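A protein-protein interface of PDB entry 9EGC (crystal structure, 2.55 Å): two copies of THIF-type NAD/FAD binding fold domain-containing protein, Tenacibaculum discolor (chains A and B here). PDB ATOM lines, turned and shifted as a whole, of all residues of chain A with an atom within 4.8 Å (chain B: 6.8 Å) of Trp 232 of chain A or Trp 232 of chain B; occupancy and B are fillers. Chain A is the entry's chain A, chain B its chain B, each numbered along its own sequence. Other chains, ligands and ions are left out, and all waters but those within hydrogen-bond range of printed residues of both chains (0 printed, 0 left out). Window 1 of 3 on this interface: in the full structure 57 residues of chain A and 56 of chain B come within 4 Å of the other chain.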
ATOM      1  N   ILE A  49      23.274  -7.335  -1.356  1.00  0.00           N
ATOM      2  CA  ILE A  49      23.890  -7.427  -2.671  1.00  0.00           C
ATOM      3  C   ILE A  49      23.271  -6.416  -3.618  1.00  0.00           C
ATOM      4  O   ILE A  49      23.981  -5.749  -4.378  1.00  0.00           O
ATOM      5  CB  ILE A  49      23.779  -8.854  -3.224  1.00  0.00           C
ATOM      6  CG1 ILE A  49      24.259  -9.859  -2.189  1.00  0.00           C
ATOM      7  CG2 ILE A  49      24.634  -8.993  -4.472  1.00  0.00           C
ATOM      8  CD1 ILE A  49      25.739  -9.673  -1.829  1.00  0.00           C
ATOM      9  N   GLU A  52      24.617  -2.688  -3.081  1.00  0.00           N
ATOM     10  CA  GLU A  52      25.930  -2.296  -3.590  1.00  0.00           C
ATOM     11  C   GLU A  52      25.878  -2.057  -5.090  1.00  0.00           C
ATOM     12  O   GLU A  52      26.334  -1.014  -5.575  1.00  0.00           O
ATOM     13  CB  GLU A  52      27.004  -3.336  -3.253  1.00  0.00           C
ATOM     14  CG  GLU A  52      28.367  -3.026  -3.928  1.00  0.00           C
ATOM     15  CD  GLU A  52      29.564  -3.780  -3.330  1.00  0.00           C
ATOM     16  OE1 GLU A  52      30.585  -3.913  -4.045  1.00  0.00           O
ATOM     17  OE2 GLU A  52      29.503  -4.213  -2.147  1.00  0.00           O
ATOM     18  N   CYS A  53      25.274  -2.991  -5.832  1.00  0.00           N
ATOM     19  CA  CYS A  53      25.175  -2.849  -7.284  1.00  0.00           C
ATOM     20  C   CYS A  53      24.423  -1.580  -7.662  1.00  0.00           C
ATOM     21  O   CYS A  53      24.783  -0.899  -8.628  1.00  0.00           O
ATOM     22  CB  CYS A  53      24.488  -4.075  -7.888  1.00  0.00           C
ATOM     23  SG  CYS A  53      24.440  -4.103  -9.717  1.00  0.00           S
ATOM     24  N   ARG A  56      26.767   1.585  -6.756  1.00  0.00           N
ATOM     25  CA  ARG A  56      27.836   1.772  -7.728  1.00  0.00           C
ATOM     26  C   ARG A  56      27.280   2.262  -9.059  1.00  0.00           C
ATOM     27  O   ARG A  56      27.929   3.065  -9.744  1.00  0.00           O
ATOM     28  CB  ARG A  56      28.620   0.471  -7.912  1.00  0.00           C
ATOM     29  CG  ARG A  56      29.364  -0.003  -6.677  1.00  0.00           C
ATOM     30  CD  ARG A  56      30.254  -1.195  -7.014  1.00  0.00           C
ATOM     31  NE  ARG A  56      30.976  -1.743  -5.864  1.00  0.00           N
ATOM     32  CZ  ARG A  56      32.113  -1.234  -5.384  1.00  0.00           C
ATOM     33  NH1 ARG A  56      32.643  -0.155  -5.947  1.00  0.00           N
ATOM     34  NH2 ARG A  56      32.724  -1.796  -4.345  1.00  0.00           N
ATOM     35  N   ARG A  77      26.239 -15.760   0.317  1.00  0.00           N
ATOM     36  CA  ARG A  77      25.443 -15.057  -0.688  1.00  0.00           C
ATOM     37  C   ARG A  77      25.077 -13.618  -0.336  1.00  0.00           C
ATOM     38  O   ARG A  77      24.411 -12.944  -1.123  1.00  0.00           O
ATOM     39  CB  ARG A  77      24.161 -15.841  -0.956  1.00  0.00           C
ATOM     40  CG  ARG A  77      23.215 -15.810   0.206  1.00  0.00           C
ATOM     41  CD  ARG A  77      22.204 -16.929   0.118  1.00  0.00           C
ATOM     42  NE  ARG A  77      21.101 -16.719   1.043  1.00  0.00           N
ATOM     43  CZ  ARG A  77      21.158 -16.980   2.341  1.00  0.00           C
ATOM     44  NH1 ARG A  77      22.272 -17.469   2.871  1.00  0.00           N
ATOM     45  NH2 ARG A  77      20.103 -16.750   3.108  1.00  0.00           N
ATOM     46  N   SER A 228      25.314 -17.877  -4.250  1.00  0.00           N
ATOM     47  CA  SER A 228      25.807 -16.550  -4.603  1.00  0.00           C
ATOM     48  C   SER A 228      25.453 -16.155  -6.034  1.00  0.00           C
ATOM     49  O   SER A 228      25.224 -14.967  -6.302  1.00  0.00           O
ATOM     50  CB  SER A 228      27.313 -16.489  -4.405  1.00  0.00           C
ATOM     51  OG  SER A 228      27.960 -17.399  -5.271  1.00  0.00           O
ATOM     52  N   VAL A 229      25.375 -17.121  -6.958  1.00  0.00           N
ATOM     53  CA  VAL A 229      25.144 -16.767  -8.358  1.00  0.00           C
ATOM     54  C   VAL A 229      23.810 -16.044  -8.512  1.00  0.00           C
ATOM     55  O   VAL A 229      23.759 -14.920  -9.023  1.00  0.00           O
ATOM     56  CB  VAL A 229      25.299 -17.997  -9.280  1.00  0.00           C
ATOM     57  CG1 VAL A 229      25.668 -19.244  -8.489  1.00  0.00           C
ATOM     58  CG2 VAL A 229      24.097 -18.218 -10.189  1.00  0.00           C
ATOM     59  N   GLY A 230      22.731 -16.618  -7.964  1.00  0.00           N
ATOM     60  CA  GLY A 230      21.433 -15.970  -8.070  1.00  0.00           C
ATOM     61  C   GLY A 230      21.393 -14.614  -7.386  1.00  0.00           C
ATOM     62  O   GLY A 230      20.753 -13.681  -7.877  1.00  0.00           O
ATOM     63  N   SER A 231      22.074 -14.484  -6.242  1.00  0.00           N
ATOM     64  CA  SER A 231      22.159 -13.191  -5.572  1.00  0.00           C
ATOM     65  C   SER A 231      22.817 -12.158  -6.473  1.00  0.00           C
ATOM     66  O   SER A 231      22.312 -11.038  -6.630  1.00  0.00           O
ATOM     67  CB  SER A 231      22.927 -13.322  -4.258  1.00  0.00           C
ATOM     68  OG  SER A 231      22.028 -13.676  -3.216  1.00  0.00           O
ATOM     69  N   TRP A 232      23.951 -12.524  -7.086  1.00  0.00           N
ATOM     70  CA  TRP A 232      24.659 -11.579  -7.943  1.00  0.00           C
ATOM     71  C   TRP A 232      23.846 -11.246  -9.184  1.00  0.00           C
ATOM     72  O   TRP A 232      23.761 -10.076  -9.584  1.00  0.00           O
ATOM     73  CB  TRP A 232      26.044 -12.132  -8.298  1.00  0.00           C
ATOM     74  CG  TRP A 232      27.114 -11.507  -7.449  1.00  0.00           C
ATOM     75  CD1 TRP A 232      28.058 -10.620  -7.859  1.00  0.00           C
ATOM     76  CD2 TRP A 232      27.292 -11.656  -6.029  1.00  0.00           C
ATOM     77  NE1 TRP A 232      28.834 -10.221  -6.793  1.00  0.00           N
ATOM     78  CE2 TRP A 232      28.392 -10.846  -5.661  1.00  0.00           C
ATOM     79  CE3 TRP A 232      26.639 -12.404  -5.037  1.00  0.00           C
ATOM     80  CZ2 TRP A 232      28.860 -10.762  -4.348  1.00  0.00           C
ATOM     81  CZ3 TRP A 232      27.099 -12.313  -3.728  1.00  0.00           C
ATOM     82  CH2 TRP A 232      28.202 -11.494  -3.398  1.00  0.00           C
ATOM     83  N   VAL A 233      23.208 -12.260  -9.776  1.00  0.00           N
ATOM     84  CA  VAL A 233      22.365 -12.047 -10.947  1.00  0.00           C
ATOM     85  C   VAL A 233      21.144 -11.204 -10.589  1.00  0.00           C
ATOM     86  O   VAL A 233      20.767 -10.294 -11.342  1.00  0.00           O
ATOM     87  CB  VAL A 233      21.981 -13.399 -11.579  1.00  0.00           C
ATOM     88  CG1 VAL A 233      20.887 -13.221 -12.632  1.00  0.00           C
ATOM     89  CG2 VAL A 233      23.203 -14.026 -12.207  1.00  0.00           C
ATOM     90  N   VAL A 234      20.499 -11.493  -9.449  1.00  0.00           N
ATOM     91  CA  VAL A 234      19.283 -10.758  -9.091  1.00  0.00           C
ATOM     92  C   VAL A 234      19.619  -9.308  -8.765  1.00  0.00           C
ATOM     93  O   VAL A 234      18.815  -8.401  -9.028  1.00  0.00           O
ATOM     94  CB  VAL A 234      18.533 -11.464  -7.935  1.00  0.00           C
ATOM     95  CG1 VAL A 234      19.058 -11.054  -6.529  1.00  0.00           C
ATOM     96  CG2 VAL A 234      17.027 -11.242  -8.052  1.00  0.00           C
ATOM     97  N   ALA A 235      20.821  -9.059  -8.227  1.00  0.00           N
ATOM     98  CA  ALA A 235      21.271  -7.692  -7.976  1.00  0.00           C
ATOM     99  C   ALA A 235      21.409  -6.907  -9.279  1.00  0.00           C
ATOM    100  O   ALA A 235      21.079  -5.717  -9.336  1.00  0.00           O
ATOM    101  CB  ALA A 235      22.590  -7.711  -7.212  1.00  0.00           C
ATOM    102  N   GLY A 236      21.924  -7.543 -10.333  1.00  0.00           N
ATOM    103  CA  GLY A 236      21.989  -6.851 -11.606  1.00  0.00           C
ATOM    104  C   GLY A 236      20.607  -6.547 -12.152  1.00  0.00           C
ATOM    105  O   GLY A 236      20.318  -5.414 -12.555  1.00  0.00           O
ATOM    106  N   ILE B  49      34.835  -8.622  -9.061  1.00  0.00           N
ATOM    107  CA  ILE B  49      33.465  -9.013  -8.762  1.00  0.00           C
ATOM    108  C   ILE B  49      33.317 -10.526  -8.871  1.00  0.00           C
ATOM    109  O   ILE B  49      32.634 -11.161  -8.053  1.00  0.00           O
ATOM    110  CB  ILE B  49      32.478  -8.296  -9.702  1.00  0.00           C
ATOM    111  CG1 ILE B  49      32.798  -6.807  -9.806  1.00  0.00           C
ATOM    112  CG2 ILE B  49      31.037  -8.468  -9.184  1.00  0.00           C
ATOM    113  CD1 ILE B  49      32.666  -6.078  -8.522  1.00  0.00           C
ATOM    114  N   ILE B  50      33.907 -11.122  -9.914  1.00  0.00           N
ATOM    115  CA  ILE B  50      33.846 -12.573 -10.075  1.00  0.00           C
ATOM    116  C   ILE B  50      34.477 -13.275  -8.877  1.00  0.00           C
ATOM    117  O   ILE B  50      33.939 -14.266  -8.360  1.00  0.00           O
ATOM    118  CB  ILE B  50      34.523 -12.988 -11.393  1.00  0.00           C
ATOM    119  CG1 ILE B  50      33.732 -12.435 -12.581  1.00  0.00           C
ATOM    120  CG2 ILE B  50      34.694 -14.509 -11.458  1.00  0.00           C
ATOM    121  CD1 ILE B  50      34.504 -12.472 -13.873  1.00  0.00           C
ATOM    122  N   GLU B  52      34.766 -12.429  -5.690  1.00  0.00           N
ATOM    123  CA  GLU B  52      33.937 -12.471  -4.485  1.00  0.00           C
ATOM    124  C   GLU B  52      32.781 -13.454  -4.639  1.00  0.00           C
ATOM    125  O   GLU B  52      32.522 -14.262  -3.739  1.00  0.00           O
ATOM    126  CB  GLU B  52      33.400 -11.086  -4.131  1.00  0.00           C
ATOM    127  CG  GLU B  52      32.405 -11.171  -2.991  1.00  0.00           C
ATOM    128  CD  GLU B  52      32.067  -9.845  -2.369  1.00  0.00           C
ATOM    129  OE1 GLU B  52      30.997  -9.759  -1.726  1.00  0.00           O
ATOM    130  OE2 GLU B  52      32.867  -8.900  -2.502  1.00  0.00           O
ATOM    131  N   CYS B  53      32.070 -13.405  -5.771  1.00  0.00           N
ATOM    132  CA  CYS B  53      30.950 -14.328  -5.972  1.00  0.00           C
ATOM    133  C   CYS B  53      31.428 -15.774  -5.967  1.00  0.00           C
ATOM    134  O   CYS B  53      30.780 -16.649  -5.378  1.00  0.00           O
ATOM    135  CB  CYS B  53      30.201 -14.003  -7.274  1.00  0.00           C
ATOM    136  SG  CYS B  53      28.660 -14.965  -7.579  1.00  0.00           S
ATOM    137  N   ALA B  54      32.574 -16.039  -6.599  1.00  0.00           N
ATOM    138  CA  ALA B  54      33.099 -17.397  -6.634  1.00  0.00           C
ATOM    139  C   ALA B  54      33.610 -17.829  -5.267  1.00  0.00           C
ATOM    140  O   ALA B  54      33.461 -19.000  -4.895  1.00  0.00           O
ATOM    141  CB  ALA B  54      34.194 -17.514  -7.690  1.00  0.00           C
ATOM    142  N   ARG B  56      32.484 -16.768  -2.230  1.00  0.00           N
ATOM    143  CA  ARG B  56      31.343 -17.023  -1.356  1.00  0.00           C
ATOM    144  C   ARG B  56      30.661 -18.334  -1.708  1.00  0.00           C
ATOM    145  O   ARG B  56      30.149 -19.021  -0.820  1.00  0.00           O
ATOM    146  CB  ARG B  56      30.353 -15.861  -1.416  1.00  0.00           C
ATOM    147  CG  ARG B  56      30.916 -14.542  -0.867  1.00  0.00           C
ATOM    148  CD  ARG B  56      29.806 -13.506  -0.782  1.00  0.00           C
ATOM    149  NE  ARG B  56      30.257 -12.208  -0.297  1.00  0.00           N
ATOM    150  CZ  ARG B  56      30.424 -11.923   0.992  1.00  0.00           C
ATOM    151  NH1 ARG B  56      30.196 -12.847   1.914  1.00  0.00           N
ATOM    152  NH2 ARG B  56      30.814 -10.715   1.372  1.00  0.00           N
ATOM    153  N   LEU B  75      35.105   2.471  -9.464  1.00  0.00           N
ATOM    154  CA  LEU B  75      34.155   2.297  -8.374  1.00  0.00           C
ATOM    155  C   LEU B  75      32.715   2.060  -8.835  1.00  0.00           C
ATOM    156  O   LEU B  75      31.874   1.703  -8.000  1.00  0.00           O
ATOM    157  CB  LEU B  75      34.228   3.504  -7.439  1.00  0.00           C
ATOM    158  CG  LEU B  75      35.586   3.800  -6.788  1.00  0.00           C
ATOM    159  CD1 LEU B  75      35.454   5.045  -5.930  1.00  0.00           C
ATOM    160  CD2 LEU B  75      36.134   2.622  -5.983  1.00  0.00           C
ATOM    161  N   ASN B  76      32.407   2.261 -10.120  1.00  0.00           N
ATOM    162  CA  ASN B  76      31.062   2.049 -10.644  1.00  0.00           C
ATOM    163  C   ASN B  76      30.758   0.592 -10.982  1.00  0.00           C
ATOM    164  O   ASN B  76      29.611   0.292 -11.338  1.00  0.00           O
ATOM    165  CB  ASN B  76      30.847   2.904 -11.900  1.00  0.00           C
ATOM    166  CG  ASN B  76      31.368   2.235 -13.173  1.00  0.00           C
ATOM    167  OD1 ASN B  76      32.424   1.608 -13.176  1.00  0.00           O
ATOM    168  ND2 ASN B  76      30.634   2.398 -14.268  1.00  0.00           N
ATOM    169  N   ARG B  77      31.746  -0.315 -10.908  1.00  0.00           N
ATOM    170  CA  ARG B  77      31.531  -1.692 -11.362  1.00  0.00           C
ATOM    171  C   ARG B  77      32.552  -2.701 -10.844  1.00  0.00           C
ATOM    172  O   ARG B  77      32.466  -3.892 -11.166  1.00  0.00           O
ATOM    173  CB  ARG B  77      31.548  -1.751 -12.889  1.00  0.00           C
ATOM    174  CG  ARG B  77      32.928  -1.484 -13.446  1.00  0.00           C
ATOM    175  CD  ARG B  77      32.859  -1.140 -14.901  1.00  0.00           C
ATOM    176  NE  ARG B  77      34.172  -1.166 -15.528  1.00  0.00           N
ATOM    177  CZ  ARG B  77      35.048  -0.167 -15.463  1.00  0.00           C
ATOM    178  NH1 ARG B  77      34.743   0.938 -14.796  1.00  0.00           N
ATOM    179  NH2 ARG B  77      36.224  -0.269 -16.078  1.00  0.00           N
ATOM    180  N   GLN B  78      33.538  -2.255 -10.082  1.00  0.00           N
ATOM    181  CA  GLN B  78      34.593  -3.141  -9.617  1.00  0.00           C
ATOM    182  C   GLN B  78      34.595  -3.175  -8.094  1.00  0.00           C
ATOM    183  O   GLN B  78      34.064  -2.283  -7.427  1.00  0.00           O
ATOM    184  CB  GLN B  78      35.967  -2.706 -10.150  1.00  0.00           C
ATOM    185  CG  GLN B  78      36.095  -2.740 -11.667  1.00  0.00           C
ATOM    186  CD  GLN B  78      37.477  -2.292 -12.158  1.00  0.00           C
ATOM    187  OE1 GLN B  78      38.427  -2.179 -11.378  1.00  0.00           O
ATOM    188  NE2 GLN B  78      37.585  -2.031 -13.454  1.00  0.00           N
ATOM    189  N   ASN B  79      35.228  -4.208  -7.550  1.00  0.00           N
ATOM    190  CA  ASN B  79      35.066  -4.561  -6.141  1.00  0.00           C
ATOM    191  C   ASN B  79      36.077  -3.796  -5.273  1.00  0.00           C
ATOM    192  O   ASN B  79      36.924  -4.363  -4.574  1.00  0.00           O
ATOM    193  CB  ASN B  79      35.198  -6.074  -5.988  1.00  0.00           C
ATOM    194  CG  ASN B  79      34.588  -6.604  -4.710  1.00  0.00           C
ATOM    195  OD1 ASN B  79      34.248  -5.845  -3.796  1.00  0.00           O
ATOM    196  ND2 ASN B  79      34.515  -7.927  -4.607  1.00  0.00           N
ATOM    197  N   ARG B  96      39.798  -7.565   0.655  1.00  0.00           N
ATOM    198  CA  ARG B  96      38.357  -7.784   0.592  1.00  0.00           C
ATOM    199  C   ARG B  96      38.019  -9.266   0.694  1.00  0.00           C
ATOM    200  O   ARG B  96      37.189  -9.670   1.518  1.00  0.00           O
ATOM    201  CB  ARG B  96      37.808  -7.182  -0.702  1.00  0.00           C
ATOM    202  CG  ARG B  96      36.390  -7.541  -0.996  1.00  0.00           C
ATOM    203  CD  ARG B  96      35.427  -6.924  -0.016  1.00  0.00           C
ATOM    204  NE  ARG B  96      34.054  -7.310  -0.346  1.00  0.00           N
ATOM    205  CZ  ARG B  96      32.996  -7.080   0.425  1.00  0.00           C
ATOM    206  NH1 ARG B  96      33.128  -6.453   1.581  1.00  0.00           N
ATOM    207  NH2 ARG B  96      31.799  -7.477   0.028  1.00  0.00           N
ATOM    208  N   ASN B 158      31.693  -7.260 -19.989  1.00  0.00           N
ATOM    209  CA  ASN B 158      30.680  -6.380 -19.415  1.00  0.00           C
ATOM    210  C   ASN B 158      29.986  -5.653 -20.563  1.00  0.00           C
ATOM    211  O   ASN B 158      30.529  -4.694 -21.117  1.00  0.00           O
ATOM    212  CB  ASN B 158      31.324  -5.411 -18.429  1.00  0.00           C
ATOM    213  CG  ASN B 158      30.311  -4.550 -17.684  1.00  0.00           C
ATOM    214  OD1 ASN B 158      29.371  -4.013 -18.269  1.00  0.00           O
ATOM    215  ND2 ASN B 158      30.520  -4.401 -16.385  1.00  0.00           N
ATOM    216  N   LEU B 227      28.767  -1.057 -16.963  1.00  0.00           N
ATOM    217  CA  LEU B 227      27.833  -0.824 -15.877  1.00  0.00           C
ATOM    218  C   LEU B 227      27.984  -1.886 -14.798  1.00  0.00           C
ATOM    219  O   LEU B 227      28.393  -3.018 -15.064  1.00  0.00           O
ATOM    220  CB  LEU B 227      26.396  -0.840 -16.397  1.00  0.00           C
ATOM    221  CG  LEU B 227      25.683   0.423 -16.870  1.00  0.00           C
ATOM    222  CD1 LEU B 227      26.625   1.572 -17.134  1.00  0.00           C
ATOM    223  CD2 LEU B 227      24.876   0.064 -18.106  1.00  0.00           C
ATOM    224  N   SER B 228      27.584  -1.527 -13.576  1.00  0.00           N
ATOM    225  CA  SER B 228      27.589  -2.503 -12.491  1.00  0.00           C
ATOM    226  C   SER B 228      26.654  -3.671 -12.778  1.00  0.00           C
ATOM    227  O   SER B 228      26.899  -4.789 -12.312  1.00  0.00           O
ATOM    228  CB  SER B 228      27.198  -1.836 -11.176  1.00  0.00           C
ATOM    229  OG  SER B 228      25.874  -1.350 -11.232  1.00  0.00           O
ATOM    230  N   VAL B 229      25.585  -3.435 -13.541  1.00  0.00           N
ATOM    231  CA  VAL B 229      24.627  -4.495 -13.845  1.00  0.00           C
ATOM    232  C   VAL B 229      25.321  -5.668 -14.517  1.00  0.00           C
ATOM    233  O   VAL B 229      25.216  -6.817 -14.068  1.00  0.00           O
ATOM    234  CB  VAL B 229      23.497  -3.958 -14.738  1.00  0.00           C
ATOM    235  CG1 VAL B 229      22.674  -5.117 -15.272  1.00  0.00           C
ATOM    236  CG2 VAL B 229      22.630  -2.950 -13.977  1.00  0.00           C
ATOM    237  N   GLY B 230      26.065  -5.387 -15.594  1.00  0.00           N
ATOM    238  CA  GLY B 230      26.731  -6.454 -16.321  1.00  0.00           C
ATOM    239  C   GLY B 230      27.806  -7.145 -15.508  1.00  0.00           C
ATOM    240  O   GLY B 230      27.961  -8.367 -15.588  1.00  0.00           O
ATOM    241  N   SER B 231      28.565  -6.375 -14.721  1.00  0.00           N
ATOM    242  CA  SER B 231      29.589  -6.968 -13.868  1.00  0.00           C
ATOM    243  C   SER B 231      28.972  -7.944 -12.876  1.00  0.00           C
ATOM    244  O   SER B 231      29.454  -9.075 -12.725  1.00  0.00           O
ATOM    245  CB  SER B 231      30.369  -5.879 -13.139  1.00  0.00           C
ATOM    246  OG  SER B 231      31.465  -5.434 -13.917  1.00  0.00           O
ATOM    247  N   TRP B 232      27.886  -7.531 -12.198  1.00  0.00           N
ATOM    248  CA  TRP B 232      27.253  -8.411 -11.219  1.00  0.00           C
ATOM    249  C   TRP B 232      26.660  -9.654 -11.883  1.00  0.00           C
ATOM    250  O   TRP B 232      26.802 -10.765 -11.361  1.00  0.00           O
ATOM    251  CB  TRP B 232      26.194  -7.646 -10.427  1.00  0.00           C
ATOM    252  CG  TRP B 232      26.690  -7.210  -9.082  1.00  0.00           C
ATOM    253  CD1 TRP B 232      26.292  -7.693  -7.876  1.00  0.00           C
ATOM    254  CD2 TRP B 232      27.724  -6.247  -8.811  1.00  0.00           C
ATOM    255  NE1 TRP B 232      26.986  -7.077  -6.868  1.00  0.00           N
ATOM    256  CE2 TRP B 232      27.868  -6.181  -7.411  1.00  0.00           C
ATOM    257  CE3 TRP B 232      28.526  -5.424  -9.617  1.00  0.00           C
ATOM    258  CZ2 TRP B 232      28.785  -5.327  -6.790  1.00  0.00           C
ATOM    259  CZ3 TRP B 232      29.437  -4.575  -9.004  1.00  0.00           C
ATOM    260  CH2 TRP B 232      29.561  -4.537  -7.599  1.00  0.00           C
ATOM    261  N   VAL B 233      26.025  -9.490 -13.052  1.00  0.00           N
ATOM    262  CA  VAL B 233      25.457 -10.630 -13.769  1.00  0.00           C
ATOM    263  C   VAL B 233      26.555 -11.577 -14.235  1.00  0.00           C
ATOM    264  O   VAL B 233      26.449 -12.802 -14.074  1.00  0.00           O
ATOM    265  CB  VAL B 233      24.602 -10.149 -14.953  1.00  0.00           C
ATOM    266  CG1 VAL B 233      24.230 -11.316 -15.850  1.00  0.00           C
ATOM    267  CG2 VAL B 233      23.351  -9.484 -14.435  1.00  0.00           C
ATOM    268  N   VAL B 234      27.630 -11.026 -14.806  1.00  0.00           N
ATOM    269  CA  VAL B 234      28.673 -11.889 -15.354  1.00  0.00           C
ATOM    270  C   VAL B 234      29.402 -12.630 -14.240  1.00  0.00           C
ATOM    271  O   VAL B 234      29.820 -13.778 -14.428  1.00  0.00           O
ATOM    272  CB  VAL B 234      29.641 -11.075 -16.256  1.00  0.00           C
ATOM    273  CG1 VAL B 234      30.767 -10.412 -15.476  1.00  0.00           C
ATOM    274  CG2 VAL B 234      30.186 -11.944 -17.371  1.00  0.00           C
ATOM    275  N   ALA B 235      29.508 -12.022 -13.049  1.00  0.00           N
ATOM    276  CA  ALA B 235      30.124 -12.704 -11.909  1.00  0.00           C
ATOM    277  C   ALA B 235      29.334 -13.948 -11.526  1.00  0.00           C
ATOM    278  O   ALA B 235      29.911 -15.005 -11.234  1.00  0.00           O
ATOM    279  CB  ALA B 235      30.219 -11.754 -10.720  1.00  0.00           C
ATOM    280  N   GLY B 236      28.004 -13.839 -11.525  1.00  0.00           N
ATOM    281  CA  GLY B 236      27.192 -15.010 -11.277  1.00  0.00           C
ATOM    282  C   GLY B 236      27.344 -16.051 -12.370  1.00  0.00           C
ATOM    283  O   GLY B 236      27.446 -17.249 -12.088  1.00  0.00           O
ATOM    284  N   MET B 237      27.352 -15.613 -13.630  1.00  0.00           N
ATOM    285  CA  MET B 237      27.521 -16.566 -14.729  1.00  0.00           C
ATOM    286  C   MET B 237      28.827 -17.325 -14.583  1.00  0.00           C
ATOM    287  O   MET B 237      28.858 -18.558 -14.696  1.00  0.00           O
ATOM    288  CB  MET B 237      27.468 -15.863 -16.086  1.00  0.00           C
ATOM    289  CG  MET B 237      26.187 -15.103 -16.329  1.00  0.00           C
ATOM    290  SD  MET B 237      26.321 -14.067 -17.786  1.00  0.00           S
ATOM    291  CE  MET B 237      26.226 -15.295 -19.078  1.00  0.00           C
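The backbone carbonyl oxygen (O) of Cys 53 of chain A sits at hydrogen-bond distance from the side-chain hydroxyl (OG) of Ser 228 of chain B, at 2.9 Å.
O of Leu 75 of chain B sits at hydrogen-bond distance from NH1 of Arg 56 of chain A, at 2.9 Å.
The backbone carbonyl oxygen (O) of Gln 78 of chain B sits at hydrogen-bond distance from the guanidinium group (NH1) of Arg 56 of chain A (3.0 Å).
The side-chain hydroxyl (OG) of Ser 228 of chain A is in hydrogen-bond range of the backbone carbonyl oxygen (O) of Cys 53 of chain B, at 2.9 Å.
OE1 of Glu 52 of chain A lies within salt-bridge range of NE of Arg 56 of chain A (2.9 Å).
The side-chain sulfur of Cys 53 of chain A is in hydrogen-bond range of the backbone carbonyl oxygen of Ala 235 of chain A, 3.7 Å away.
The side-chain carboxylate (OE1) of Glu 52 of chain B is in salt-bridge range of the guanidinium group (NE) of Arg 56 of chain B.
The side-chain amide nitrogen (ND2) of Asn 79 of chain B lies within hydrogen-bond range of the side-chain carboxylate (OE2) of Glu 52 of chain B, 2.8 Å away.
The side-chain amide oxygen of Asn 76 of chain B lies within hydrogen-bond range of the guanidinium group of Arg 77 of chain B, at 2.9 Å.
The side-chain amide nitrogen (NE2) of Gln 78 of chain B sits close to the guanidinium group (NH2) of Arg 77 of chain B (3.4 Å).
Trp 232 of chain B touches Glu 52 of chain A.
CH2 of Trp 232 of chain B touches CD of Arg 56 of chain A, at 3.5 Å.
Val 229 of chain A touches Cys 53 of chain B (N to SG, 3.98 Å).
O of Gly 236 of chain B touches CB of Val 229 of chain A, 3.6 Å away.
CG2 of Ile 49 of chain B touches NE1 of Trp 232 of chain A, 3.7 Å away.
Trp 232 of chain A touches Glu 52 of chain B.
Trp 232 of chain A touches Cys 53 of chain B (CG to SG, 3.8 Å).
Trp 232 of chain B touches Trp 232 of chain A.
CB of Ala 235 of chain A touches CD1 of Trp 232 of chain B (3.8 Å).
CG1 of Val 229 of chain B touches O of Gly 236 of chain A, at 3.6 Å.
Of the printed residues of chain B, Cys 53 of chain A touches Ser 228 (2.9 Å) and Trp 232 (3.9 Å).
Of the printed residues of chain B, Arg 56 of chain A touches Leu 75 (2.9 Å), Asn 76 (3.4 Å), Gln 78 (3.0 Å) and Trp 232 (3.5 Å).
Printed residues of chain B within 4 Å of Trp 232 of chain A: Ile 49 (3.7 Å), Glu 52 (3.5 Å), Cys 53 (3.8 Å), Arg 56 (3.7 Å), Trp 232 (3.4 Å) and Ala 235 (3.8 Å).
Printed residues of chain B within 4 Å of Gly 236 of chain A: Val 229 (3.6 Å).
Printed residues of chain A within 4 Å of Leu 75 of chain B: Arg 56.
Asn 79 of chain B touches none of the printed residues of chain A.
Trp 232 of chain B touches six residues of chain A.
Printed residues of chain A within 4 Å of Ala 235 of chain B: Trp 232.
Met 237 of chain B touches none of the printed residues of chain A.
The nearest residue of chain B that does not touch Trp 232 of chain A is Gly 236 of chain B (4.1 Å).
The nearest printed residue of chain B that does not touch Val 233 of chain A is Trp 232 of chain B (4.2 Å).
Printed residues of chain A that touch a printed residue of chain B: Ile 49, Glu 52, Cys 53, Arg 56, Ser 228, Val 229, Trp 232, Val 233, Ala 235 and Gly 236.
Hydrophobic or aromatic side chains of chain A that line the printed part of chain B: Ile 49, Val 229, Trp 232, Val 233 and Ala 235.
Along chain A the printed residues that touch a printed residue of chain B span positions 49 to 236.
Of the 24 printed residues of chain B, 13 touch a printed residue of chain A.
Hydrophobic or aromatic side chains of chain B within 4 Å of the printed part of chain A: Ile 49, Val 229, Trp 232 and Ala 235.
Cys 53 of chain A touches Ser 228 of chain B, and with the chains exchanged Ser 228 of chain A touches Cys 53 of chain B.
Arg 56 of chain A touches Trp 232 of chain B, and with the chains exchanged Trp 232 of chain A touches Arg 56 of chain B.
Val 229 of chain A touches Cys 53 of chain B, but with the chains exchanged Cys 53 of chain A does not touch Val 229 of chain B (4.05 Å).
Val 229 of chain A touches Gly 236 of chain B, and with the chains exchanged Gly 236 of chain A touches Val 229 of chain B.
Positions printed for both chains: 49, 52, 53, 56, 77, 228, 229, 230, 231, 232, 233, 234, 235 and 236.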
